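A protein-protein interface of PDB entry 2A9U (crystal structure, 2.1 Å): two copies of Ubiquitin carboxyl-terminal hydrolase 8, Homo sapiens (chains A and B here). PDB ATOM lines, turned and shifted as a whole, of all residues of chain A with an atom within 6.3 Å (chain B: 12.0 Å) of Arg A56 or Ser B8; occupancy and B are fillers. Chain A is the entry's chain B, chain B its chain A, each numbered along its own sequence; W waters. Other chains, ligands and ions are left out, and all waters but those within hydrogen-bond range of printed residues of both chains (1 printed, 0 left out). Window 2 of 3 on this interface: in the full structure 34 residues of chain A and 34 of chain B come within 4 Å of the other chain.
No position is printed for both chains.
Of the 13 pairs that touch across the chains among the printed residues, none has its exchanged pair printed and touching as well.
Among the printed residues, pairs that only touch across the chains: Asp A57 with Lys B11, Arg A56 with Pro B10, Glu A59 with Leu B13, Arg A114 with Pro B10, Arg A114 with Leu B13, Arg A56 with Val B9 and Asp A55 with Lys B11.
Of the printed residues of chain B, Arg A56 touches Ser B8, Val B9, Pro B10 and Lys B11.
Of chain A, only Arg A56 comes within 4 Å of Ser B8.
Cys A52 touches none of the printed residues of chain B.
Of chain B, only Lys B11 (3.97 Å) comes within 4 Å of Asp A55.
Printed residues of chain A within 4 Å of Leu B15: Glu A59.
Of the printed residues of chain A, Pro B10 touches Arg A56 (3.6 Å) and Arg A114 (3.6 Å).
The nearest printed residue of chain B that does not touch Arg A114 is Glu B12 (4.2 Å).
Water W1 lies within hydrogen-bond range of O of Lys B11 (2.9 Å), NH1 of Arg A114 (2.9 Å) and N of Glu A58 (3.1 Å).
Hydrophobic or aromatic side chains of chain B that line the printed part of chain A: Pro B10, Leu B13, Tyr B14 and Leu B15.
Among the printed residues, 13 pairs touch across the chains.
Among the printed residues, no Asp or Glu carboxylate lies within 4 Å of a Lys or Arg side-chain nitrogen of the other chain.
The guanidinium group (NE) of Arg A56 lies within hydrogen-bond range of the side-chain hydroxyl (OG) of Ser B8, at 2.8 Å.
The backbone carbonyl oxygen (O) of Arg A56 is in hydrogen-bond range of the backbone NH (N) of Lys B11 (3.0 Å).
The backbone NH (N) of Leu B15 lies within hydrogen-bond range of the side-chain carboxylate (OE1) of Glu A59 (2.9 Å).
The side-chain hydroxyl (OH) of Tyr B14 lies within hydrogen-bond range of the side-chain carboxylate (OD2) of Asp A57, 2.5 Å away.
O of Lys B11 is in hydrogen-bond range of NH2 of Arg A114 (2.8 Å).
OE1 of Glu A59 sits at hydrogen-bond distance from N of Tyr B14 (2.9 Å).
The side-chain carboxylate of Glu A58 is in salt-bridge range of the guanidinium group of Arg A114 (2.8 Å).
O of Cys A52 is in hydrogen-bond range of N of Asp A57, at 3.0 Å.
The side-chain carboxylate of Glu A58 lies within salt-bridge range of the guanidinium group of Arg A56 (3.6 Å).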
ATOM      1  N   GLU A  51      10.629  -6.783  33.947  1.00  0.00           N
ATOM      2  CA  GLU A  51      10.112  -7.936  34.681  1.00  0.00           C
ATOM      3  C   GLU A  51       9.163  -8.775  33.854  1.00  0.00           C
ATOM      4  O   GLU A  51       9.241  -9.988  33.889  1.00  0.00           O
ATOM      5  CB  GLU A  51       9.398  -7.497  35.960  1.00  0.00           C
ATOM      6  CG  GLU A  51      10.355  -7.082  37.085  1.00  0.00           C
ATOM      7  CD  GLU A  51       9.698  -6.192  38.152  1.00  0.00           C
ATOM      8  OE1 GLU A  51       8.458  -6.155  38.280  1.00  0.00           O
ATOM      9  OE2 GLU A  51      10.441  -5.501  38.864  1.00  0.00           O
ATOM     10  N   CYS A  52       8.236  -8.139  33.143  1.00  0.00           N
ATOM     11  CA  CYS A  52       7.298  -8.871  32.297  1.00  0.00           C
ATOM     12  C   CYS A  52       8.034  -9.598  31.187  1.00  0.00           C
ATOM     13  O   CYS A  52       7.706 -10.754  30.904  1.00  0.00           O
ATOM     14  CB  CYS A  52       6.251  -7.948  31.691  1.00  0.00           C
ATOM     15  SG  CYS A  52       5.092  -7.324  32.855  1.00  0.00           S
ATOM     16  N   ARG A  53       9.003  -8.924  30.557  1.00  0.00           N
ATOM     17  CA  ARG A  53       9.807  -9.547  29.492  1.00  0.00           C
ATOM     18  C   ARG A  53      10.556 -10.784  30.016  1.00  0.00           C
ATOM     19  O   ARG A  53      10.586 -11.844  29.381  1.00  0.00           O
ATOM     20  CB  ARG A  53      10.799  -8.567  28.883  1.00  0.00           C
ATOM     21  CG  ARG A  53      11.597  -9.161  27.679  1.00  0.00           C
ATOM     22  CD  ARG A  53      12.671  -8.214  27.199  1.00  0.00           C
ATOM     23  NE  ARG A  53      13.422  -7.686  28.331  1.00  0.00           N
ATOM     24  CZ  ARG A  53      14.687  -7.991  28.616  1.00  0.00           C
ATOM     25  NH1 ARG A  53      15.385  -8.802  27.827  1.00  0.00           N
ATOM     26  NH2 ARG A  53      15.264  -7.472  29.684  1.00  0.00           N
ATOM     27  N   LEU A  54      11.159 -10.642  31.184  1.00  0.00           N
ATOM     28  CA  LEU A  54      11.870 -11.758  31.800  1.00  0.00           C
ATOM     29  C   LEU A  54      10.903 -12.870  32.174  1.00  0.00           C
ATOM     30  O   LEU A  54      11.263 -14.036  32.123  1.00  0.00           O
ATOM     31  CB  LEU A  54      12.658 -11.274  33.023  1.00  0.00           C
ATOM     32  CG  LEU A  54      13.912 -10.522  32.562  1.00  0.00           C
ATOM     33  CD1 LEU A  54      14.389  -9.474  33.573  1.00  0.00           C
ATOM     34  CD2 LEU A  54      15.014 -11.509  32.251  1.00  0.00           C
ATOM     35  N   ASP A  55       9.666 -12.500  32.518  1.00  0.00           N
ATOM     36  CA  ASP A  55       8.647 -13.468  32.863  1.00  0.00           C
ATOM     37  C   ASP A  55       7.958 -14.046  31.604  1.00  0.00           C
ATOM     38  O   ASP A  55       7.077 -14.895  31.701  1.00  0.00           O
ATOM     39  CB  ASP A  55       7.632 -12.817  33.790  1.00  0.00           C
ATOM     40  CG  ASP A  55       6.790 -13.820  34.530  1.00  0.00           C
ATOM     41  OD1 ASP A  55       7.338 -14.534  35.400  1.00  0.00           O
ATOM     42  OD2 ASP A  55       5.569 -13.898  34.251  1.00  0.00           O
ATOM     43  N   ARG A  56       8.355 -13.588  30.427  1.00  0.00           N
ATOM     44  CA  ARG A  56       7.820 -14.127  29.157  1.00  0.00           C
ATOM     45  C   ARG A  56       6.394 -13.676  28.811  1.00  0.00           C
ATOM     46  O   ARG A  56       5.749 -14.288  27.979  1.00  0.00           O
ATOM     47  CB  ARG A  56       7.904 -15.671  29.115  1.00  0.00           C
ATOM     48  CG  ARG A  56       9.292 -16.267  29.451  1.00  0.00           C
ATOM     49  CD  ARG A  56      10.406 -15.764  28.517  1.00  0.00           C
ATOM     50  NE  ARG A  56      10.489 -16.600  27.323  1.00  0.00           N
ATOM     51  CZ  ARG A  56      10.088 -16.237  26.108  1.00  0.00           C
ATOM     52  NH1 ARG A  56       9.576 -15.024  25.897  1.00  0.00           N
ATOM     53  NH2 ARG A  56      10.206 -17.094  25.097  1.00  0.00           N
ATOM     54  N   ASP A  57       5.906 -12.618  29.454  1.00  0.00           N
ATOM     55  CA  ASP A  57       4.606 -12.011  29.125  1.00  0.00           C
ATOM     56  C   ASP A  57       4.838 -10.988  28.036  1.00  0.00           C
ATOM     57  O   ASP A  57       5.053  -9.805  28.308  1.00  0.00           O
ATOM     58  CB  ASP A  57       3.984 -11.309  30.341  1.00  0.00           C
ATOM     59  CG  ASP A  57       2.517 -10.957  30.123  1.00  0.00           C
ATOM     60  OD1 ASP A  57       2.074 -10.836  28.958  1.00  0.00           O
ATOM     61  OD2 ASP A  57       1.793 -10.834  31.132  1.00  0.00           O
ATOM     62  N   GLU A  58       4.806 -11.450  26.793  1.00  0.00           N
ATOM     63  CA  GLU A  58       5.132 -10.589  25.675  1.00  0.00           C
ATOM     64  C   GLU A  58       4.149  -9.425  25.458  1.00  0.00           C
ATOM     65  O   GLU A  58       4.567  -8.316  25.160  1.00  0.00           O
ATOM     66  CB  GLU A  58       5.292 -11.431  24.416  1.00  0.00           C
ATOM     67  CG  GLU A  58       6.449 -12.443  24.484  1.00  0.00           C
ATOM     68  CD  GLU A  58       6.766 -13.063  23.127  1.00  0.00           C
ATOM     69  OE1 GLU A  58       5.943 -12.915  22.190  1.00  0.00           O
ATOM     70  OE2 GLU A  58       7.853 -13.668  22.995  1.00  0.00           O
ATOM     71  N   GLU A  59       2.849  -9.671  25.613  1.00  0.00           N
ATOM     72  CA  GLU A  59       1.832  -8.608  25.479  1.00  0.00           C
ATOM     73  C   GLU A  59       1.991  -7.508  26.529  1.00  0.00           C
ATOM     74  O   GLU A  59       1.989  -6.329  26.172  1.00  0.00           O
ATOM     75  CB  GLU A  59       0.413  -9.187  25.588  1.00  0.00           C
ATOM     76  CG  GLU A  59       0.038 -10.187  24.482  1.00  0.00           C
ATOM     77  CD  GLU A  59      -1.299 -10.848  24.768  1.00  0.00           C
ATOM     78  OE1 GLU A  59      -1.381 -11.571  25.816  1.00  0.00           O
ATOM     79  OE2 GLU A  59      -2.258 -10.628  23.958  1.00  0.00           O
ATOM     80  N   ARG A 106      11.003  -5.537  18.726  1.00  0.00           N
ATOM     81  CA  ARG A 106      11.187  -6.981  18.711  1.00  0.00           C
ATOM     82  C   ARG A 106       9.901  -7.689  19.155  1.00  0.00           C
ATOM     83  O   ARG A 106       9.487  -8.659  18.523  1.00  0.00           O
ATOM     84  CB  ARG A 106      12.345  -7.364  19.627  1.00  0.00           C
ATOM     85  CG  ARG A 106      12.599  -8.867  19.678  1.00  0.00           C
ATOM     86  CD  ARG A 106      13.688  -9.246  20.710  1.00  0.00           C
ATOM     87  NE  ARG A 106      13.222  -9.262  22.112  1.00  0.00           N
ATOM     88  CZ  ARG A 106      12.264 -10.054  22.619  1.00  0.00           C
ATOM     89  NH1 ARG A 106      11.596 -10.914  21.852  1.00  0.00           N
ATOM     90  NH2 ARG A 106      11.947  -9.970  23.913  1.00  0.00           N
ATOM     91  N   ARG A 114       2.259 -14.083  16.317  1.00  0.00           N
ATOM     92  CA  ARG A 114       1.533 -14.895  17.255  1.00  0.00           C
ATOM     93  C   ARG A 114       0.020 -14.638  17.116  1.00  0.00           C
ATOM     94  O   ARG A 114      -0.780 -15.583  17.224  1.00  0.00           O
ATOM     95  CB  ARG A 114       2.048 -14.663  18.682  1.00  0.00           C
ATOM     96  CG  ARG A 114       3.530 -15.076  18.878  1.00  0.00           C
ATOM     97  CD  ARG A 114       3.979 -14.942  20.331  1.00  0.00           C
ATOM     98  NE  ARG A 114       3.184 -15.738  21.281  1.00  0.00           N
ATOM     99  CZ  ARG A 114       3.066 -15.442  22.578  1.00  0.00           C
ATOM    100  NH1 ARG A 114       3.734 -14.403  23.070  1.00  0.00           N
ATOM    101  NH2 ARG A 114       2.323 -16.188  23.387  1.00  0.00           N
ATOM    102  N   SER B   8      12.402 -22.101  26.927  1.00  0.00           N
ATOM    103  CA  SER B   8      11.594 -21.002  27.534  1.00  0.00           C
ATOM    104  C   SER B   8      10.430 -20.548  26.628  1.00  0.00           C
ATOM    105  O   SER B   8      10.628 -19.821  25.644  1.00  0.00           O
ATOM    106  CB  SER B   8      12.489 -19.821  27.891  1.00  0.00           C
ATOM    107  OG  SER B   8      11.723 -18.789  28.477  1.00  0.00           O
ATOM    108  N   VAL B   9       9.216 -20.978  26.983  1.00  0.00           N
ATOM    109  CA  VAL B   9       8.015 -20.750  26.174  1.00  0.00           C
ATOM    110  C   VAL B   9       7.334 -19.463  26.684  1.00  0.00           C
ATOM    111  O   VAL B   9       7.357 -19.213  27.900  1.00  0.00           O
ATOM    112  CB  VAL B   9       7.078 -22.022  26.220  1.00  0.00           C
ATOM    113  CG1 VAL B   9       6.487 -22.246  27.626  1.00  0.00           C
ATOM    114  CG2 VAL B   9       5.977 -21.985  25.139  1.00  0.00           C
ATOM    115  N   PRO B  10       6.768 -18.625  25.766  1.00  0.00           N
ATOM    116  CA  PRO B  10       6.115 -17.402  26.251  1.00  0.00           C
ATOM    117  C   PRO B  10       4.778 -17.747  26.874  1.00  0.00           C
ATOM    118  O   PRO B  10       4.185 -18.747  26.507  1.00  0.00           O
ATOM    119  CB  PRO B  10       5.909 -16.563  24.991  1.00  0.00           C
ATOM    120  CG  PRO B  10       6.471 -17.350  23.858  1.00  0.00           C
ATOM    121  CD  PRO B  10       6.700 -18.743  24.297  1.00  0.00           C
ATOM    122  N   LYS B  11       4.318 -16.952  27.831  1.00  0.00           N
ATOM    123  CA  LYS B  11       2.964 -17.109  28.363  1.00  0.00           C
ATOM    124  C   LYS B  11       1.953 -17.142  27.221  1.00  0.00           C
ATOM    125  O   LYS B  11       2.138 -16.460  26.188  1.00  0.00           O
ATOM    126  CB  LYS B  11       2.624 -15.952  29.319  1.00  0.00           C
ATOM    127  CG  LYS B  11       2.818 -16.262  30.800  1.00  0.00           C
ATOM    128  CD  LYS B  11       2.754 -14.999  31.675  1.00  0.00           C
ATOM    129  CE  LYS B  11       1.431 -14.219  31.522  1.00  0.00           C
ATOM    130  NZ  LYS B  11       0.242 -14.787  32.241  1.00  0.00           N
ATOM    131  N   GLU B  12       0.897 -17.940  27.389  1.00  0.00           N
ATOM    132  CA  GLU B  12      -0.197 -17.987  26.406  1.00  0.00           C
ATOM    133  C   GLU B  12      -0.748 -16.573  26.254  1.00  0.00           C
ATOM    134  O   GLU B  12      -0.829 -15.828  27.230  1.00  0.00           O
ATOM    135  CB  GLU B  12      -1.346 -18.904  26.873  1.00  0.00           C
ATOM    136  CG  GLU B  12      -1.281 -20.357  26.465  1.00  0.00           C
ATOM    137  CD  GLU B  12      -2.518 -21.121  26.967  1.00  0.00           C
ATOM    138  OE1 GLU B  12      -2.359 -22.062  27.793  1.00  0.00           O
ATOM    139  OE2 GLU B  12      -3.656 -20.758  26.554  1.00  0.00           O
ATOM    140  N   LEU B  13      -1.143 -16.236  25.035  1.00  0.00           N
ATOM    141  CA  LEU B  13      -1.798 -14.967  24.736  1.00  0.00           C
ATOM    142  C   LEU B  13      -3.068 -14.864  25.560  1.00  0.00           C
ATOM    143  O   LEU B  13      -3.776 -15.852  25.720  1.00  0.00           O
ATOM    144  CB  LEU B  13      -2.123 -14.875  23.245  1.00  0.00           C
ATOM    145  CG  LEU B  13      -0.923 -14.719  22.286  1.00  0.00           C
ATOM    146  CD1 LEU B  13      -1.398 -14.676  20.847  1.00  0.00           C
ATOM    147  CD2 LEU B  13      -0.079 -13.464  22.597  1.00  0.00           C
ATOM    148  N   TYR B  14      -3.338 -13.682  26.109  1.00  0.00           N
ATOM    149  CA  TYR B  14      -4.491 -13.498  26.996  1.00  0.00           C
ATOM    150  C   TYR B  14      -5.022 -12.076  26.976  1.00  0.00           C
ATOM    151  O   TYR B  14      -6.190 -11.840  27.275  1.00  0.00           O
ATOM    152  CB  TYR B  14      -4.122 -13.894  28.446  1.00  0.00           C
ATOM    153  CG  TYR B  14      -3.199 -12.913  29.168  1.00  0.00           C
ATOM    154  CD1 TYR B  14      -3.726 -11.895  29.999  1.00  0.00           C
ATOM    155  CD2 TYR B  14      -1.804 -12.984  29.004  1.00  0.00           C
ATOM    156  CE1 TYR B  14      -2.868 -10.962  30.657  1.00  0.00           C
ATOM    157  CE2 TYR B  14      -0.958 -12.080  29.642  1.00  0.00           C
ATOM    158  CZ  TYR B  14      -1.494 -11.075  30.475  1.00  0.00           C
ATOM    159  OH  TYR B  14      -0.633 -10.193  31.086  1.00  0.00           O
ATOM    160  N   LEU B  15      -4.167 -11.125  26.648  1.00  0.00           N
ATOM    161  CA  LEU B  15      -4.490  -9.720  26.890  1.00  0.00           C
ATOM    162  C   LEU B  15      -5.233  -9.109  25.708  1.00  0.00           C
ATOM    163  O   LEU B  15      -6.048  -8.207  25.864  1.00  0.00           O
ATOM    164  CB  LEU B  15      -3.196  -8.948  27.191  1.00  0.00           C
ATOM    165  CG  LEU B  15      -3.191  -7.596  27.890  1.00  0.00           C
ATOM    166  CD1 LEU B  15      -3.987  -7.614  29.212  1.00  0.00           C
ATOM    167  CD2 LEU B  15      -1.721  -7.170  28.142  1.00  0.00           C
ATOM    168  N   LEU B  22      -4.176  -4.159  21.214  1.00  0.00           N
ATOM    169  CA  LEU B  22      -3.108  -4.044  22.213  1.00  0.00           C
ATOM    170  C   LEU B  22      -2.515  -2.645  22.224  1.00  0.00           C
ATOM    171  O   LEU B  22      -2.266  -2.108  23.289  1.00  0.00           O
ATOM    172  CB  LEU B  22      -2.016  -5.086  21.930  1.00  0.00           C
ATOM    173  CG  LEU B  22      -1.111  -5.487  23.083  1.00  0.00           C
ATOM    174  CD1 LEU B  22      -1.898  -6.062  24.290  1.00  0.00           C
ATOM    175  CD2 LEU B  22      -0.039  -6.468  22.545  1.00  0.00           C
HETATM  176  O   HOH W   1       3.013 -13.712  25.806  1.00  0.00           O
